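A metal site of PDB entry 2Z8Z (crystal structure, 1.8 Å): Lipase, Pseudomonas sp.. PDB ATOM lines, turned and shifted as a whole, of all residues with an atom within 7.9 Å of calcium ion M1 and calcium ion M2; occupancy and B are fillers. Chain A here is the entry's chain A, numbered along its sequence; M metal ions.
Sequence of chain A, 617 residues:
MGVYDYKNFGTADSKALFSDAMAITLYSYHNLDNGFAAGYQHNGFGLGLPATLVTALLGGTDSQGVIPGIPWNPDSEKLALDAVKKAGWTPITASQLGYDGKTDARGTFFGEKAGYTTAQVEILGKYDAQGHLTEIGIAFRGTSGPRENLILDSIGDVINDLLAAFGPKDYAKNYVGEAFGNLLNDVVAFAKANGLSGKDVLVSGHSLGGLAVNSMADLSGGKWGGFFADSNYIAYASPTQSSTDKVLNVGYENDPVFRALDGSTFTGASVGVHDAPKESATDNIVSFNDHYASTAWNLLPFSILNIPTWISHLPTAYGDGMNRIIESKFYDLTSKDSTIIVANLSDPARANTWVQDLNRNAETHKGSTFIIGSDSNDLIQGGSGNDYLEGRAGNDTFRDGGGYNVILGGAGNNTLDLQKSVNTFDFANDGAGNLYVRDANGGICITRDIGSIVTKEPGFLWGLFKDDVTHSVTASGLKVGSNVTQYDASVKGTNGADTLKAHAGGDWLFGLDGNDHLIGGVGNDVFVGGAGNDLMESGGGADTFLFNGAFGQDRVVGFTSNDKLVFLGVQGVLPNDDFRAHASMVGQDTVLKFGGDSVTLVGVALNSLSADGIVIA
Residues that only touch calcium ion M2: Gly 410 (3.9 Å). Within 4 Å of calcium ion M2: Arg 392, Ala 393, Gly 394, Asp 396, Gly 409, Gly 410, Ala 411 and Asn 414. The nearest printed residue that does not touch calcium ion M2 is Gly 391 (4.2 Å).
The backbone carbonyl oxygen (O) of Asp 378 is in hydrogen-bond range of the backbone NH (N) of Thr 397, at 2.9 Å. The backbone NH (N) of Thr 415 is in hydrogen-bond range of the backbone carbonyl oxygen (O) of Asp 396, at 2.9 Å. N of Ser 376 is in hydrogen-bond range of OG of Ser 374, 3.0 Å away. The backbone NH (N) of Gly 391 lies within hydrogen-bond range of the backbone carbonyl oxygen (O) of Leu 408 (3.0 Å). The guanidinium group (NE) of Arg 392 lies within salt-bridge range of the side-chain carboxylate (OD1) of Asp 375, 2.9 Å away. The side-chain amide nitrogen (ND2) of Asn 414 is in hydrogen-bond range of the backbone carbonyl oxygen (O) of Gly 410, at 3.1 Å. The backbone carbonyl oxygen of Gly 412 is in hydrogen-bond range of the side-chain amide nitrogen of Asn 414 (3.4 Å). ND2 of Asn 414 lies within hydrogen-bond range of O of Asp 449 (2.8 Å).
Calcium ion M2 is bound by OD2 of Asp 396 (2.3 Å), O of Ala 411 (2.3 Å), O of Gly 394 (2.3 Å), O of Arg 392 (2.3 Å), O of Gly 409 (2.4 Å) and OD1 of Asn 414 (2.5 Å).
Calcium ion M1 is bound by OD2 of Asp 378 (2.2 Å), O of Ala 393 (2.2 Å), O of Ser 376 (2.3 Å), O of Gly 391 (2.3 Å), O of Ser 374 (2.4 Å) and OD1 of Asp 396 (2.5 Å). Calcium ion M1 has six donor atoms within binding distance. Slightly farther from calcium ion M1 lies the side-chain carboxylate (OD2) of Asp 396 (3.0 Å).
Of the 30 residues printed, 7 come within 4 Å of calcium ion M1.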
ATOM      1  N   ALA A 343      25.352  12.910 -13.798  1.00  0.00           N
ATOM      2  CA  ALA A 343      25.673  12.552 -15.145  1.00  0.00           C
ATOM      3  C   ALA A 343      27.190  12.358 -15.271  1.00  0.00           C
ATOM      4  O   ALA A 343      27.974  13.346 -15.259  1.00  0.00           O
ATOM      5  CB  ALA A 343      25.195  13.645 -16.097  1.00  0.00           C
ATOM      6  N   ARG A 350      27.457  10.062 -24.037  1.00  0.00           N
ATOM      7  CA  ARG A 350      26.621  11.213 -23.694  1.00  0.00           C
ATOM      8  C   ARG A 350      25.725  11.592 -24.868  1.00  0.00           C
ATOM      9  O   ARG A 350      24.589  12.108 -24.687  1.00  0.00           O
ATOM     10  CB  ARG A 350      27.504  12.414 -23.302  1.00  0.00           C
ATOM     11  CG  ARG A 350      26.706  13.534 -22.672  1.00  0.00           C
ATOM     12  CD  ARG A 350      27.604  14.640 -22.200  1.00  0.00           C
ATOM     13  NE  ARG A 350      28.520  15.048 -23.256  1.00  0.00           N
ATOM     14  CZ  ARG A 350      29.843  15.019 -23.198  1.00  0.00           C
ATOM     15  NH1 ARG A 350      30.488  14.638 -22.105  1.00  0.00           N
ATOM     16  NH2 ARG A 350      30.524  15.429 -24.258  1.00  0.00           N
ATOM     17  N   ILE A 372      21.642  15.756 -12.005  1.00  0.00           N
ATOM     18  CA  ILE A 372      22.607  16.824 -12.243  1.00  0.00           C
ATOM     19  C   ILE A 372      23.392  16.552 -13.528  1.00  0.00           C
ATOM     20  O   ILE A 372      24.136  15.572 -13.628  1.00  0.00           O
ATOM     21  CB  ILE A 372      23.628  16.950 -11.081  1.00  0.00           C
ATOM     22  CG1 ILE A 372      22.917  17.028  -9.723  1.00  0.00           C
ATOM     23  CG2 ILE A 372      24.471  18.211 -11.211  1.00  0.00           C
ATOM     24  CD1 ILE A 372      21.867  18.030  -9.688  1.00  0.00           C
ATOM     25  N   GLY A 373      23.314  17.479 -14.454  1.00  0.00           N
ATOM     26  CA  GLY A 373      24.025  17.331 -15.736  1.00  0.00           C
ATOM     27  C   GLY A 373      25.507  17.642 -15.718  1.00  0.00           C
ATOM     28  O   GLY A 373      26.076  17.927 -14.668  1.00  0.00           O
ATOM     29  N   SER A 374      26.148  17.587 -16.907  1.00  0.00           N
ATOM     30  CA  SER A 374      27.544  17.956 -17.113  1.00  0.00           C
ATOM     31  C   SER A 374      27.593  19.301 -17.767  1.00  0.00           C
ATOM     32  O   SER A 374      26.568  19.834 -18.185  1.00  0.00           O
ATOM     33  CB  SER A 374      28.251  16.978 -18.042  1.00  0.00           C
ATOM     34  OG  SER A 374      27.816  17.086 -19.380  1.00  0.00           O
ATOM     35  N   ASP A 375      28.788  19.828 -17.926  1.00  0.00           N
ATOM     36  CA  ASP A 375      28.943  21.054 -18.660  1.00  0.00           C
ATOM     37  C   ASP A 375      28.868  20.926 -20.176  1.00  0.00           C
ATOM     38  O   ASP A 375      29.006  21.945 -20.877  1.00  0.00           O
ATOM     39  CB  ASP A 375      30.194  21.740 -18.188  1.00  0.00           C
ATOM     40  CG  ASP A 375      29.966  22.440 -16.840  1.00  0.00           C
ATOM     41  OD1 ASP A 375      28.829  22.900 -16.519  1.00  0.00           O
ATOM     42  OD2 ASP A 375      30.926  22.554 -16.171  1.00  0.00           O
ATOM     43  N   SER A 376      28.591  19.729 -20.660  1.00  0.00           N
ATOM     44  CA  SER A 376      28.389  19.524 -22.099  1.00  0.00           C
ATOM     45  C   SER A 376      26.912  19.260 -22.415  1.00  0.00           C
ATOM     46  O   SER A 376      26.011  19.410 -21.549  1.00  0.00           O
ATOM     47  CB  SER A 376      29.266  18.378 -22.542  1.00  0.00           C
ATOM     48  OG  SER A 376      30.617  18.655 -22.204  1.00  0.00           O
ATOM     49  N   ASN A 377      26.625  18.920 -23.673  1.00  0.00           N
ATOM     50  CA  ASN A 377      25.263  18.657 -24.095  1.00  0.00           C
ATOM     51  C   ASN A 377      24.752  17.344 -23.538  1.00  0.00           C
ATOM     52  O   ASN A 377      25.289  16.288 -23.900  1.00  0.00           O
ATOM     53  CB  ASN A 377      25.231  18.539 -25.635  1.00  0.00           C
ATOM     54  CG  ASN A 377      25.634  19.805 -26.304  1.00  0.00           C
ATOM     55  OD1 ASN A 377      25.921  20.765 -25.650  1.00  0.00           O
ATOM     56  ND2 ASN A 377      25.637  19.803 -27.644  1.00  0.00           N
ATOM     57  N   ASP A 378      23.737  17.416 -22.672  1.00  0.00           N
ATOM     58  CA  ASP A 378      23.152  16.246 -22.012  1.00  0.00           C
ATOM     59  C   ASP A 378      21.754  15.945 -22.529  1.00  0.00           C
ATOM     60  O   ASP A 378      21.061  16.872 -22.941  1.00  0.00           O
ATOM     61  CB  ASP A 378      23.042  16.566 -20.492  1.00  0.00           C
ATOM     62  CG  ASP A 378      24.389  16.912 -19.876  1.00  0.00           C
ATOM     63  OD1 ASP A 378      25.299  16.044 -19.987  1.00  0.00           O
ATOM     64  OD2 ASP A 378      24.549  18.040 -19.288  1.00  0.00           O
ATOM     65  N   LEU A 379      21.347  14.666 -22.425  1.00  0.00           N
ATOM     66  CA  LEU A 379      19.995  14.133 -22.592  1.00  0.00           C
ATOM     67  C   LEU A 379      19.632  13.677 -21.186  1.00  0.00           C
ATOM     68  O   LEU A 379      20.272  12.789 -20.632  1.00  0.00           O
ATOM     69  CB  LEU A 379      19.926  12.912 -23.565  1.00  0.00           C
ATOM     70  CG  LEU A 379      20.543  13.212 -24.945  1.00  0.00           C
ATOM     71  CD1 LEU A 379      20.605  11.960 -25.786  1.00  0.00           C
ATOM     72  CD2 LEU A 379      19.749  14.281 -25.635  1.00  0.00           C
ATOM     73  N   ILE A 380      18.675  14.392 -20.597  1.00  0.00           N
ATOM     74  CA  ILE A 380      18.236  14.156 -19.230  1.00  0.00           C
ATOM     75  C   ILE A 380      16.752  13.730 -19.176  1.00  0.00           C
ATOM     76  O   ILE A 380      15.854  14.438 -19.673  1.00  0.00           O
ATOM     77  CB  ILE A 380      18.518  15.413 -18.370  1.00  0.00           C
ATOM     78  CG1 ILE A 380      20.047  15.666 -18.239  1.00  0.00           C
ATOM     79  CG2 ILE A 380      17.885  15.271 -17.028  1.00  0.00           C
ATOM     80  CD1 ILE A 380      20.427  16.949 -17.684  1.00  0.00           C
ATOM     81  N   GLU A 390      18.806  19.479 -13.775  1.00  0.00           N
ATOM     82  CA  GLU A 390      19.724  20.610 -13.921  1.00  0.00           C
ATOM     83  C   GLU A 390      20.699  20.303 -15.068  1.00  0.00           C
ATOM     84  O   GLU A 390      21.485  19.354 -15.001  1.00  0.00           O
ATOM     85  CB  GLU A 390      20.498  20.857 -12.615  1.00  0.00           C
ATOM     86  CG  GLU A 390      21.402  22.090 -12.713  1.00  0.00           C
ATOM     87  CD  GLU A 390      22.055  22.436 -11.390  1.00  0.00           C
ATOM     88  OE1 GLU A 390      22.522  21.436 -10.717  1.00  0.00           O
ATOM     89  OE2 GLU A 390      22.127  23.656 -11.056  1.00  0.00           O
ATOM     90  N   GLY A 391      20.609  21.114 -16.123  1.00  0.00           N
ATOM     91  CA  GLY A 391      21.414  20.959 -17.325  1.00  0.00           C
ATOM     92  C   GLY A 391      22.842  21.469 -17.242  1.00  0.00           C
ATOM     93  O   GLY A 391      23.721  20.849 -17.847  1.00  0.00           O
ATOM     94  N   ARG A 392      23.069  22.520 -16.462  1.00  0.00           N
ATOM     95  CA  ARG A 392      24.302  23.262 -16.478  1.00  0.00           C
ATOM     96  C   ARG A 392      24.632  23.697 -17.931  1.00  0.00           C
ATOM     97  O   ARG A 392      23.719  23.825 -18.715  1.00  0.00           O
ATOM     98  CB  ARG A 392      25.457  22.450 -15.822  1.00  0.00           C
ATOM     99  CG  ARG A 392      25.173  21.930 -14.405  1.00  0.00           C
ATOM    100  CD  ARG A 392      26.397  21.094 -13.842  1.00  0.00           C
ATOM    101  NE  ARG A 392      27.670  21.802 -14.079  1.00  0.00           N
ATOM    102  CZ  ARG A 392      28.301  22.539 -13.163  1.00  0.00           C
ATOM    103  NH1 ARG A 392      27.796  22.663 -11.954  1.00  0.00           N
ATOM    104  NH2 ARG A 392      29.464  23.088 -13.403  1.00  0.00           N
ATOM    105  N   ALA A 393      25.905  23.956 -18.255  1.00  0.00           N
ATOM    106  CA  ALA A 393      26.243  24.430 -19.578  1.00  0.00           C
ATOM    107  C   ALA A 393      26.011  23.362 -20.598  1.00  0.00           C
ATOM    108  O   ALA A 393      25.669  22.147 -20.285  1.00  0.00           O
ATOM    109  CB  ALA A 393      27.687  24.922 -19.609  1.00  0.00           C
ATOM    110  N   GLY A 394      26.159  23.762 -21.859  1.00  0.00           N
ATOM    111  CA  GLY A 394      25.875  22.848 -22.926  1.00  0.00           C
ATOM    112  C   GLY A 394      24.400  22.961 -23.302  1.00  0.00           C
ATOM    113  O   GLY A 394      23.581  23.557 -22.574  1.00  0.00           O
ATOM    114  N   ASN A 395      24.086  22.467 -24.489  1.00  0.00           N
ATOM    115  CA  ASN A 395      22.740  22.508 -25.062  1.00  0.00           C
ATOM    116  C   ASN A 395      22.120  21.211 -24.575  1.00  0.00           C
ATOM    117  O   ASN A 395      22.452  20.136 -25.053  1.00  0.00           O
ATOM    118  CB  ASN A 395      22.789  22.481 -26.566  1.00  0.00           C
ATOM    119  CG  ASN A 395      23.360  23.773 -27.155  1.00  0.00           C
ATOM    120  OD1 ASN A 395      23.522  24.767 -26.456  1.00  0.00           O
ATOM    121  ND2 ASN A 395      23.700  23.732 -28.451  1.00  0.00           N
ATOM    122  N   ASP A 396      21.195  21.326 -23.620  1.00  0.00           N
ATOM    123  CA  ASP A 396      20.639  20.127 -22.953  1.00  0.00           C
ATOM    124  C   ASP A 396      19.233  19.892 -23.422  1.00  0.00           C
ATOM    125  O   ASP A 396      18.494  20.852 -23.621  1.00  0.00           O
ATOM    126  CB  ASP A 396      20.651  20.351 -21.414  1.00  0.00           C
ATOM    127  CG  ASP A 396      22.035  20.636 -20.922  1.00  0.00           C
ATOM    128  OD1 ASP A 396      22.889  19.782 -21.236  1.00  0.00           O
ATOM    129  OD2 ASP A 396      22.304  21.730 -20.365  1.00  0.00           O
ATOM    130  N   THR A 397      18.852  18.603 -23.519  1.00  0.00           N
ATOM    131  CA  THR A 397      17.517  18.227 -23.868  1.00  0.00           C
ATOM    132  C   THR A 397      16.886  17.438 -22.711  1.00  0.00           C
ATOM    133  O   THR A 397      17.528  16.519 -22.206  1.00  0.00           O
ATOM    134  CB  THR A 397      17.483  17.380 -25.136  1.00  0.00           C
ATOM    135  OG1 THR A 397      18.112  18.141 -26.196  1.00  0.00           O
ATOM    136  CG2 THR A 397      16.082  17.119 -25.500  1.00  0.00           C
ATOM    137  N   PHE A 398      15.694  17.866 -22.289  1.00  0.00           N
ATOM    138  CA  PHE A 398      14.994  17.231 -21.165  1.00  0.00           C
ATOM    139  C   PHE A 398      13.721  16.547 -21.593  1.00  0.00           C
ATOM    140  O   PHE A 398      12.967  17.045 -22.422  1.00  0.00           O
ATOM    141  CB  PHE A 398      14.638  18.252 -20.088  1.00  0.00           C
ATOM    142  CG  PHE A 398      15.797  19.051 -19.572  1.00  0.00           C
ATOM    143  CD1 PHE A 398      16.494  18.668 -18.442  1.00  0.00           C
ATOM    144  CD2 PHE A 398      16.179  20.223 -20.210  1.00  0.00           C
ATOM    145  CE1 PHE A 398      17.585  19.493 -17.966  1.00  0.00           C
ATOM    146  CE2 PHE A 398      17.216  20.993 -19.745  1.00  0.00           C
ATOM    147  CZ  PHE A 398      17.932  20.614 -18.593  1.00  0.00           C
ATOM    148  N   LEU A 408      15.950  23.301 -14.897  1.00  0.00           N
ATOM    149  CA  LEU A 408      16.836  24.448 -15.083  1.00  0.00           C
ATOM    150  C   LEU A 408      17.724  24.159 -16.306  1.00  0.00           C
ATOM    151  O   LEU A 408      18.640  23.378 -16.253  1.00  0.00           O
ATOM    152  CB  LEU A 408      17.696  24.708 -13.875  1.00  0.00           C
ATOM    153  CG  LEU A 408      16.917  24.954 -12.540  1.00  0.00           C
ATOM    154  CD1 LEU A 408      17.855  25.098 -11.338  1.00  0.00           C
ATOM    155  CD2 LEU A 408      16.100  26.217 -12.736  1.00  0.00           C
ATOM    156  N   GLY A 409      17.439  24.824 -17.399  1.00  0.00           N
ATOM    157  CA  GLY A 409      18.281  24.645 -18.549  1.00  0.00           C
ATOM    158  C   GLY A 409      19.734  25.027 -18.402  1.00  0.00           C
ATOM    159  O   GLY A 409      20.569  24.458 -19.109  1.00  0.00           O
ATOM    160  N   GLY A 410      20.034  26.022 -17.568  1.00  0.00           N
ATOM    161  CA  GLY A 410      21.361  26.640 -17.486  1.00  0.00           C
ATOM    162  C   GLY A 410      21.784  27.370 -18.749  1.00  0.00           C
ATOM    163  O   GLY A 410      20.938  27.747 -19.587  1.00  0.00           O
ATOM    164  N   ALA A 411      23.083  27.593 -18.893  1.00  0.00           N
ATOM    165  CA  ALA A 411      23.663  28.115 -20.110  1.00  0.00           C
ATOM    166  C   ALA A 411      23.335  27.268 -21.294  1.00  0.00           C
ATOM    167  O   ALA A 411      22.914  26.128 -21.188  1.00  0.00           O
ATOM    168  CB  ALA A 411      25.168  28.267 -19.968  1.00  0.00           C
ATOM    169  N   GLY A 412      23.484  27.832 -22.478  1.00  0.00           N
ATOM    170  CA  GLY A 412      23.209  27.085 -23.708  1.00  0.00           C
ATOM    171  C   GLY A 412      21.811  27.263 -24.313  1.00  0.00           C
ATOM    172  O   GLY A 412      20.965  27.995 -23.792  1.00  0.00           O
ATOM    173  N   ASN A 413      21.597  26.559 -25.418  1.00  0.00           N
ATOM    174  CA  ASN A 413      20.283  26.492 -26.066  1.00  0.00           C
ATOM    175  C   ASN A 413      19.670  25.174 -25.685  1.00  0.00           C
ATOM    176  O   ASN A 413      20.083  24.107 -26.191  1.00  0.00           O
ATOM    177  CB  ASN A 413      20.414  26.579 -27.588  1.00  0.00           C
ATOM    178  CG  ASN A 413      21.022  27.865 -28.026  1.00  0.00           C
ATOM    179  OD1 ASN A 413      20.708  28.950 -27.511  1.00  0.00           O
ATOM    180  ND2 ASN A 413      21.963  27.762 -28.969  1.00  0.00           N
ATOM    181  N   ASN A 414      18.688  25.246 -24.793  1.00  0.00           N
ATOM    182  CA  ASN A 414      18.112  24.072 -24.192  1.00  0.00           C
ATOM    183  C   ASN A 414      16.701  23.793 -24.689  1.00  0.00           C
ATOM    184  O   ASN A 414      15.988  24.725 -25.021  1.00  0.00           O
ATOM    185  CB  ASN A 414      18.096  24.223 -22.632  1.00  0.00           C
ATOM    186  CG  ASN A 414      19.421  24.700 -22.096  1.00  0.00           C
ATOM    187  OD1 ASN A 414      20.404  23.981 -22.172  1.00  0.00           O
ATOM    188  ND2 ASN A 414      19.450  25.930 -21.546  1.00  0.00           N
ATOM    189  N   THR A 415      16.297  22.534 -24.616  1.00  0.00           N
ATOM    190  CA  THR A 415      15.047  22.027 -25.118  1.00  0.00           C
ATOM    191  C   THR A 415      14.308  21.115 -24.126  1.00  0.00           C
ATOM    192  O   THR A 415      14.908  20.274 -23.457  1.00  0.00           O
ATOM    193  CB  THR A 415      15.362  21.182 -26.397  1.00  0.00           C
ATOM    194  OG1 THR A 415      16.037  22.048 -27.329  1.00  0.00           O
ATOM    195  CG2 THR A 415      14.097  20.636 -27.061  1.00  0.00           C
ATOM    196  N   ASP A 449      15.376  29.015 -18.651  1.00  0.00           N
ATOM    197  CA  ASP A 449      16.398  28.918 -19.714  1.00  0.00           C
ATOM    198  C   ASP A 449      16.098  27.806 -20.698  1.00  0.00           C
ATOM    199  O   ASP A 449      16.988  27.209 -21.212  1.00  0.00           O
ATOM    200  CB  ASP A 449      17.784  28.766 -19.052  1.00  0.00           C
ATOM    201  CG  ASP A 449      18.121  29.957 -18.176  1.00  0.00           C
ATOM    202  OD1 ASP A 449      18.098  31.086 -18.697  1.00  0.00           O
ATOM    203  OD2 ASP A 449      18.376  29.812 -16.983  1.00  0.00           O
ATOM    204  N   ILE A 450      14.826  27.606 -21.009  1.00  0.00           N
ATOM    205  CA  ILE A 450      14.444  26.651 -22.028  1.00  0.00           C
ATOM    206  C   ILE A 450      13.839  27.471 -23.197  1.00  0.00           C
ATOM    207  O   ILE A 450      12.808  28.133 -23.047  1.00  0.00           O
ATOM    208  CB  ILE A 450      13.582  25.500 -21.445  1.00  0.00           C
ATOM    209  CG1 ILE A 450      14.596  24.521 -20.753  1.00  0.00           C
ATOM    210  CG2 ILE A 450      12.758  24.871 -22.623  1.00  0.00           C
ATOM    211  CD1 ILE A 450      14.122  23.503 -19.856  1.00  0.00           C
HETATM  212 CA    CA M   1      24.819  20.163 -19.762  1.00  0.00          CA
HETATM  213 CA    CA M   2      22.375  23.984 -20.634  1.00  0.00          CA
